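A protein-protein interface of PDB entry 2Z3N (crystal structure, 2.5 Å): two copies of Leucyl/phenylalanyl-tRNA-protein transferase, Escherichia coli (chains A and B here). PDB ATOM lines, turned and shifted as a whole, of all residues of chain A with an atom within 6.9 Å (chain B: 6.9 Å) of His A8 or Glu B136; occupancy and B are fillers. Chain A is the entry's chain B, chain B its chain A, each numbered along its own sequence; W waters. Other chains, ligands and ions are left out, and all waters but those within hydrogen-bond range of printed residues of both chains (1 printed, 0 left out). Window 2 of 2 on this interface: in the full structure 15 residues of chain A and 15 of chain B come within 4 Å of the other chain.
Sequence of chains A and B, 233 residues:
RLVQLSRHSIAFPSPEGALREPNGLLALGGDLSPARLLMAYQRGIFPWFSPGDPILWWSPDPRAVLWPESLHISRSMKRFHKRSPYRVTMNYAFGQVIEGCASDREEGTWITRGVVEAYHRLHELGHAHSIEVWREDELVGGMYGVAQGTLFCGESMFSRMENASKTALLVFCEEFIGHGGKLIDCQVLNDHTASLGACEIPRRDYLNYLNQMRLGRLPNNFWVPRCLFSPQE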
ATOM      1  N   LEU A   5      17.614 -29.884  13.691  1.00  0.00           N
ATOM      2  CA  LEU A   5      18.555 -28.774  13.735  1.00  0.00           C
ATOM      3  C   LEU A   5      19.579 -28.828  14.860  1.00  0.00           C
ATOM      4  O   LEU A   5      19.360 -29.467  15.891  1.00  0.00           O
ATOM      5  CB  LEU A   5      17.767 -27.467  13.823  1.00  0.00           C
ATOM      6  CG  LEU A   5      16.578 -27.415  12.863  1.00  0.00           C
ATOM      7  CD1 LEU A   5      15.711 -26.221  13.170  1.00  0.00           C
ATOM      8  CD2 LEU A   5      17.086 -27.370  11.433  1.00  0.00           C
ATOM      9  N   SER A   6      20.697 -28.138  14.639  1.00  0.00           N
ATOM     10  CA  SER A   6      21.788 -28.047  15.610  1.00  0.00           C
ATOM     11  C   SER A   6      21.912 -26.578  15.975  1.00  0.00           C
ATOM     12  O   SER A   6      21.333 -25.732  15.300  1.00  0.00           O
ATOM     13  CB  SER A   6      23.105 -28.500  14.985  1.00  0.00           C
ATOM     14  OG  SER A   6      23.545 -27.562  14.016  1.00  0.00           O
ATOM     15  N   ARG A   7      22.660 -26.268  17.031  1.00  0.00           N
ATOM     16  CA  ARG A   7      22.838 -24.874  17.413  1.00  0.00           C
ATOM     17  C   ARG A   7      23.897 -24.280  16.492  1.00  0.00           C
ATOM     18  O   ARG A   7      24.033 -23.063  16.365  1.00  0.00           O
ATOM     19  CB  ARG A   7      23.300 -24.759  18.860  1.00  0.00           C
ATOM     20  CG  ARG A   7      23.306 -23.318  19.357  1.00  0.00           C
ATOM     21  CD  ARG A   7      24.114 -23.159  20.635  1.00  0.00           C
ATOM     22  NE  ARG A   7      24.151 -21.766  21.080  1.00  0.00           N
ATOM     23  CZ  ARG A   7      24.992 -21.294  21.998  1.00  0.00           C
ATOM     24  NH1 ARG A   7      25.876 -22.102  22.577  1.00  0.00           N
ATOM     25  NH2 ARG A   7      24.955 -20.009  22.335  1.00  0.00           N
ATOM     26  N   HIS A   8      24.634 -25.166  15.833  1.00  0.00           N
ATOM     27  CA  HIS A   8      25.696 -24.774  14.917  1.00  0.00           C
ATOM     28  C   HIS A   8      25.214 -24.040  13.663  1.00  0.00           C
ATOM     29  O   HIS A   8      25.979 -23.314  13.036  1.00  0.00           O
ATOM     30  CB  HIS A   8      26.506 -26.015  14.512  1.00  0.00           C
ATOM     31  CG  HIS A   8      27.168 -26.706  15.663  1.00  0.00           C
ATOM     32  ND1 HIS A   8      27.853 -27.893  15.523  1.00  0.00           N
ATOM     33  CD2 HIS A   8      27.256 -26.375  16.974  1.00  0.00           C
ATOM     34  CE1 HIS A   8      28.334 -28.265  16.697  1.00  0.00           C
ATOM     35  NE2 HIS A   8      27.986 -27.360  17.595  1.00  0.00           N
ATOM     36  N   SER A   9      23.959 -24.228  13.275  1.00  0.00           N
ATOM     37  CA  SER A   9      23.464 -23.537  12.089  1.00  0.00           C
ATOM     38  C   SER A   9      22.054 -22.993  12.270  1.00  0.00           C
ATOM     39  O   SER A   9      21.217 -23.594  12.943  1.00  0.00           O
ATOM     40  CB  SER A   9      23.505 -24.459  10.868  1.00  0.00           C
ATOM     41  OG  SER A   9      23.031 -23.783   9.712  1.00  0.00           O
ATOM     42  N   ILE A  10      21.803 -21.847  11.655  1.00  0.00           N
ATOM     43  CA  ILE A  10      20.508 -21.199  11.736  1.00  0.00           C
ATOM     44  C   ILE A  10      19.747 -21.497  10.438  1.00  0.00           C
ATOM     45  O   ILE A  10      18.647 -20.991  10.202  1.00  0.00           O
ATOM     46  CB  ILE A  10      20.713 -19.663  11.982  1.00  0.00           C
ATOM     47  CG1 ILE A  10      19.886 -19.222  13.179  1.00  0.00           C
ATOM     48  CG2 ILE A  10      20.345 -18.843  10.777  1.00  0.00           C
ATOM     49  CD1 ILE A  10      20.303 -19.880  14.453  1.00  0.00           C
ATOM     50  N   ALA A  11      20.334 -22.358   9.613  1.00  0.00           N
ATOM     51  CA  ALA A  11      19.745 -22.736   8.330  1.00  0.00           C
ATOM     52  C   ALA A  11      18.572 -23.716   8.424  1.00  0.00           C
ATOM     53  O   ALA A  11      18.614 -24.686   9.182  1.00  0.00           O
ATOM     54  CB  ALA A  11      20.825 -23.319   7.423  1.00  0.00           C
ATOM     55  N   SER A  33      16.187 -18.392  19.318  1.00  0.00           N
ATOM     56  CA  SER A  33      17.009 -17.190  19.250  1.00  0.00           C
ATOM     57  C   SER A  33      16.449 -16.238  18.204  1.00  0.00           C
ATOM     58  O   SER A  33      15.903 -16.664  17.188  1.00  0.00           O
ATOM     59  CB  SER A  33      18.450 -17.533  18.867  1.00  0.00           C
ATOM     60  OG  SER A  33      18.546 -17.881  17.493  1.00  0.00           O
ATOM     61  N   ALA A  35      17.716 -14.650  15.844  1.00  0.00           N
ATOM     62  CA  ALA A  35      18.214 -14.880  14.489  1.00  0.00           C
ATOM     63  C   ALA A  35      17.534 -16.054  13.807  1.00  0.00           C
ATOM     64  O   ALA A  35      17.333 -16.044  12.585  1.00  0.00           O
ATOM     65  CB  ALA A  35      19.731 -15.097  14.509  1.00  0.00           C
ATOM     66  N   ARG A  36      17.186 -17.068  14.590  1.00  0.00           N
ATOM     67  CA  ARG A  36      16.538 -18.236  14.023  1.00  0.00           C
ATOM     68  C   ARG A  36      15.086 -17.921  13.695  1.00  0.00           C
ATOM     69  O   ARG A  36      14.612 -18.229  12.595  1.00  0.00           O
ATOM     70  CB  ARG A  36      16.604 -19.411  14.989  1.00  0.00           C
ATOM     71  CG  ARG A  36      16.988 -20.711  14.307  1.00  0.00           C
ATOM     72  CD  ARG A  36      16.775 -21.900  15.212  1.00  0.00           C
ATOM     73  NE  ARG A  36      17.855 -22.870  15.065  1.00  0.00           N
ATOM     74  CZ  ARG A  36      19.027 -22.761  15.675  1.00  0.00           C
ATOM     75  NH1 ARG A  36      19.259 -21.730  16.470  1.00  0.00           N
ATOM     76  NH2 ARG A  36      19.966 -23.670  15.493  1.00  0.00           N
ATOM     77  N   PRO B  85      32.172 -16.895   7.044  1.00  0.00           N
ATOM     78  CA  PRO B  85      31.383 -17.678   7.994  1.00  0.00           C
ATOM     79  C   PRO B  85      30.271 -16.777   8.562  1.00  0.00           C
ATOM     80  O   PRO B  85      29.510 -17.185   9.438  1.00  0.00           O
ATOM     81  CB  PRO B  85      32.409 -18.026   9.055  1.00  0.00           C
ATOM     82  CG  PRO B  85      33.174 -16.731   9.160  1.00  0.00           C
ATOM     83  CD  PRO B  85      33.397 -16.382   7.690  1.00  0.00           C
ATOM     84  N   TYR B  86      30.191 -15.550   8.048  1.00  0.00           N
ATOM     85  CA  TYR B  86      29.221 -14.577   8.535  1.00  0.00           C
ATOM     86  C   TYR B  86      28.011 -14.306   7.658  1.00  0.00           C
ATOM     87  O   TYR B  86      28.035 -14.469   6.432  1.00  0.00           O
ATOM     88  CB  TYR B  86      29.915 -13.241   8.798  1.00  0.00           C
ATOM     89  CG  TYR B  86      31.025 -13.309   9.823  1.00  0.00           C
ATOM     90  CD1 TYR B  86      32.188 -12.555   9.665  1.00  0.00           C
ATOM     91  CD2 TYR B  86      30.916 -14.126  10.955  1.00  0.00           C
ATOM     92  CE1 TYR B  86      33.214 -12.613  10.598  1.00  0.00           C
ATOM     93  CE2 TYR B  86      31.938 -14.190  11.899  1.00  0.00           C
ATOM     94  CZ  TYR B  86      33.089 -13.432  11.711  1.00  0.00           C
ATOM     95  OH  TYR B  86      34.128 -13.500  12.619  1.00  0.00           O
ATOM     96  N   ARG B  87      26.947 -13.885   8.323  1.00  0.00           N
ATOM     97  CA  ARG B  87      25.718 -13.511   7.662  1.00  0.00           C
ATOM     98  C   ARG B  87      25.536 -12.047   8.060  1.00  0.00           C
ATOM     99  O   ARG B  87      25.867 -11.650   9.191  1.00  0.00           O
ATOM    100  CB  ARG B  87      24.559 -14.353   8.187  1.00  0.00           C
ATOM    101  CG  ARG B  87      23.724 -14.991   7.102  1.00  0.00           C
ATOM    102  CD  ARG B  87      22.863 -16.085   7.690  1.00  0.00           C
ATOM    103  NE  ARG B  87      22.793 -17.263   6.828  1.00  0.00           N
ATOM    104  CZ  ARG B  87      23.000 -18.509   7.255  1.00  0.00           C
ATOM    105  NH1 ARG B  87      23.295 -18.732   8.536  1.00  0.00           N
ATOM    106  NH2 ARG B  87      22.899 -19.530   6.408  1.00  0.00           N
ATOM    107  N   TRP B 134      26.277 -11.844  11.894  1.00  0.00           N
ATOM    108  CA  TRP B 134      25.986 -13.070  12.619  1.00  0.00           C
ATOM    109  C   TRP B 134      26.882 -14.233  12.262  1.00  0.00           C
ATOM    110  O   TRP B 134      27.210 -14.473  11.106  1.00  0.00           O
ATOM    111  CB  TRP B 134      24.547 -13.556  12.373  1.00  0.00           C
ATOM    112  CG  TRP B 134      23.484 -12.522  12.486  1.00  0.00           C
ATOM    113  CD1 TRP B 134      23.043 -11.684  11.503  1.00  0.00           C
ATOM    114  CD2 TRP B 134      22.747 -12.187  13.666  1.00  0.00           C
ATOM    115  NE1 TRP B 134      22.073 -10.838  12.002  1.00  0.00           N
ATOM    116  CE2 TRP B 134      21.875 -11.127  13.327  1.00  0.00           C
ATOM    117  CE3 TRP B 134      22.743 -12.678  14.978  1.00  0.00           C
ATOM    118  CZ2 TRP B 134      21.011 -10.547  14.252  1.00  0.00           C
ATOM    119  CZ3 TRP B 134      21.882 -12.098  15.903  1.00  0.00           C
ATOM    120  CH2 TRP B 134      21.026 -11.039  15.530  1.00  0.00           C
ATOM    121  N   ARG B 135      27.261 -14.965  13.284  1.00  0.00           N
ATOM    122  CA  ARG B 135      28.048 -16.151  13.100  1.00  0.00           C
ATOM    123  C   ARG B 135      27.025 -17.172  13.584  1.00  0.00           C
ATOM    124  O   ARG B 135      26.817 -17.322  14.786  1.00  0.00           O
ATOM    125  CB  ARG B 135      29.287 -16.106  14.001  1.00  0.00           C
ATOM    126  CG  ARG B 135      30.119 -17.371  13.987  1.00  0.00           C
ATOM    127  CD  ARG B 135      30.394 -17.862  12.571  1.00  0.00           C
ATOM    128  NE  ARG B 135      30.891 -19.232  12.630  1.00  0.00           N
ATOM    129  CZ  ARG B 135      30.742 -20.135  11.669  1.00  0.00           C
ATOM    130  NH1 ARG B 135      30.111 -19.820  10.548  1.00  0.00           N
ATOM    131  NH2 ARG B 135      31.192 -21.369  11.853  1.00  0.00           N
ATOM    132  N   GLU B 136      26.354 -17.830  12.642  1.00  0.00           N
ATOM    133  CA  GLU B 136      25.329 -18.813  12.977  1.00  0.00           C
ATOM    134  C   GLU B 136      24.186 -18.068  13.685  1.00  0.00           C
ATOM    135  O   GLU B 136      23.589 -17.159  13.112  1.00  0.00           O
ATOM    136  CB  GLU B 136      25.909 -19.906  13.891  1.00  0.00           C
ATOM    137  CG  GLU B 136      27.106 -20.673  13.302  1.00  0.00           C
ATOM    138  CD  GLU B 136      27.870 -21.526  14.344  1.00  0.00           C
ATOM    139  OE1 GLU B 136      28.378 -20.953  15.343  1.00  0.00           O
ATOM    140  OE2 GLU B 136      27.977 -22.767  14.165  1.00  0.00           O
ATOM    141  N   ASP B 137      23.915 -18.437  14.935  1.00  0.00           N
ATOM    142  CA  ASP B 137      22.849 -17.825  15.728  1.00  0.00           C
ATOM    143  C   ASP B 137      23.330 -16.698  16.626  1.00  0.00           C
ATOM    144  O   ASP B 137      22.517 -16.033  17.273  1.00  0.00           O
ATOM    145  CB  ASP B 137      22.190 -18.875  16.613  1.00  0.00           C
ATOM    146  CG  ASP B 137      23.137 -19.425  17.657  1.00  0.00           C
ATOM    147  OD1 ASP B 137      24.219 -19.919  17.286  1.00  0.00           O
ATOM    148  OD2 ASP B 137      22.799 -19.364  18.854  1.00  0.00           O
ATOM    149  N   GLU B 138      24.641 -16.477  16.667  1.00  0.00           N
ATOM    150  CA  GLU B 138      25.197 -15.438  17.524  1.00  0.00           C
ATOM    151  C   GLU B 138      25.564 -14.110  16.857  1.00  0.00           C
ATOM    152  O   GLU B 138      26.222 -14.077  15.816  1.00  0.00           O
ATOM    153  CB  GLU B 138      26.425 -15.986  18.246  1.00  0.00           C
ATOM    154  CG  GLU B 138      27.100 -15.009  19.196  1.00  0.00           C
ATOM    155  CD  GLU B 138      28.301 -15.627  19.903  1.00  0.00           C
ATOM    156  OE1 GLU B 138      28.133 -16.687  20.546  1.00  0.00           O
ATOM    157  OE2 GLU B 138      29.410 -15.060  19.824  1.00  0.00           O
ATOM    158  N   LEU B 139      25.123 -13.018  17.475  1.00  0.00           N
ATOM    159  CA  LEU B 139      25.433 -11.678  16.994  1.00  0.00           C
ATOM    160  C   LEU B 139      26.908 -11.446  17.366  1.00  0.00           C
ATOM    161  O   LEU B 139      27.244 -11.341  18.548  1.00  0.00           O
ATOM    162  CB  LEU B 139      24.556 -10.646  17.705  1.00  0.00           C
ATOM    163  CG  LEU B 139      24.808  -9.211  17.247  1.00  0.00           C
ATOM    164  CD1 LEU B 139      24.460  -9.096  15.762  1.00  0.00           C
ATOM    165  CD2 LEU B 139      23.981  -8.240  18.082  1.00  0.00           C
ATOM    166  N   VAL B 140      27.784 -11.355  16.368  1.00  0.00           N
ATOM    167  CA  VAL B 140      29.204 -11.202  16.646  1.00  0.00           C
ATOM    168  C   VAL B 140      29.797  -9.876  16.223  1.00  0.00           C
ATOM    169  O   VAL B 140      31.003  -9.683  16.291  1.00  0.00           O
ATOM    170  CB  VAL B 140      29.991 -12.318  15.973  1.00  0.00           C
ATOM    171  CG1 VAL B 140      29.488 -13.645  16.467  1.00  0.00           C
ATOM    172  CG2 VAL B 140      29.844 -12.217  14.464  1.00  0.00           C
ATOM    173  N   MET B 161      34.260 -11.100  17.017  1.00  0.00           N
ATOM    174  CA  MET B 161      34.892 -12.183  16.273  1.00  0.00           C
ATOM    175  C   MET B 161      35.718 -11.591  15.132  1.00  0.00           C
ATOM    176  O   MET B 161      35.342 -10.578  14.547  1.00  0.00           O
ATOM    177  CB  MET B 161      33.815 -13.135  15.737  1.00  0.00           C
ATOM    178  CG  MET B 161      34.269 -14.575  15.506  1.00  0.00           C
ATOM    179  SD  MET B 161      32.843 -15.688  15.405  1.00  0.00           S
ATOM    180  CE  MET B 161      33.567 -17.139  14.607  1.00  0.00           C
HETATM  181  O   HOH W   1      19.936 -14.710  17.737  1.00  0.00           O
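No position is printed for both chains.
Of the 7 pairs that touch across the chains among the printed residues, none has its exchanged pair printed and touching as well.
Among the printed residues, merely in contact across the chains: Ile A10 with Arg B87 (3.7 Å), Ile A10 with Glu B136 (3.98 Å), Ile A10 with Asp B137 (3.0 Å), Ser A33 with Asp B137 (3.9 Å) and Ala A35 with Trp B134 (3.9 Å).
The backbone carbonyl oxygen of Arg B87 is in hydrogen-bond range of the backbone NH of Trp B134, 2.7 Å away.
OG of Ser A33 lies within hydrogen-bond range of N of Arg A36, 3.3 Å away.
OG of Ser A6 sits close to N of His A8.
Water W1 lies within hydrogen-bond range of N of Ala A35, O of Asp B137 and OG of Ser A33.
Of chain B, only Glu B136 comes within 4 Å of His A8.
Of the printed residues of chain B, Ser A33 touches Asp B137 (3.9 Å).
Printed residues of chain B within 4 Å of Ala A35: Trp B134.
Pro B85 touches none of the printed residues of chain A.
Of the printed residues of chain A, Asp B137 touches Arg A7 (3.3 Å), Ile A10 (3.0 Å) and Ser A33 (3.9 Å).
Val B140 touches none of the printed residues of chain A.
The nearest residue of chain B that does not touch His A8 is Asp B137 (5.5 Å).
The nearest printed residue of chain B that does not touch Ile A10 is Glu B138 (5.9 Å).
Of the 11 printed residues of chain B, 4 touch a printed residue of chain A.
Hydrophobic or aromatic side chains of chain B that line the printed part of chain A: Trp B134.
Of the 10 printed residues of chain A, 5 touch a printed residue of chain B.
Printed residues of chain A that touch a printed residue of chain B: Arg A7, His A8, Ile A10, Ser A33 and Ala A35.
Among the printed residues, Asp or Glu carboxylates within 4 Å of a Lys or Arg side-chain nitrogen of the other chain: Arg A7 with Asp B137 (3.5 Å).
OE2 of Glu B136 lies close to O of His A8, at 2.4 Å.
The guanidinium group (NE) of Arg A7 lies within salt-bridge range of the side-chain carboxylate (OD2) of Asp B137 (3.5 Å).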
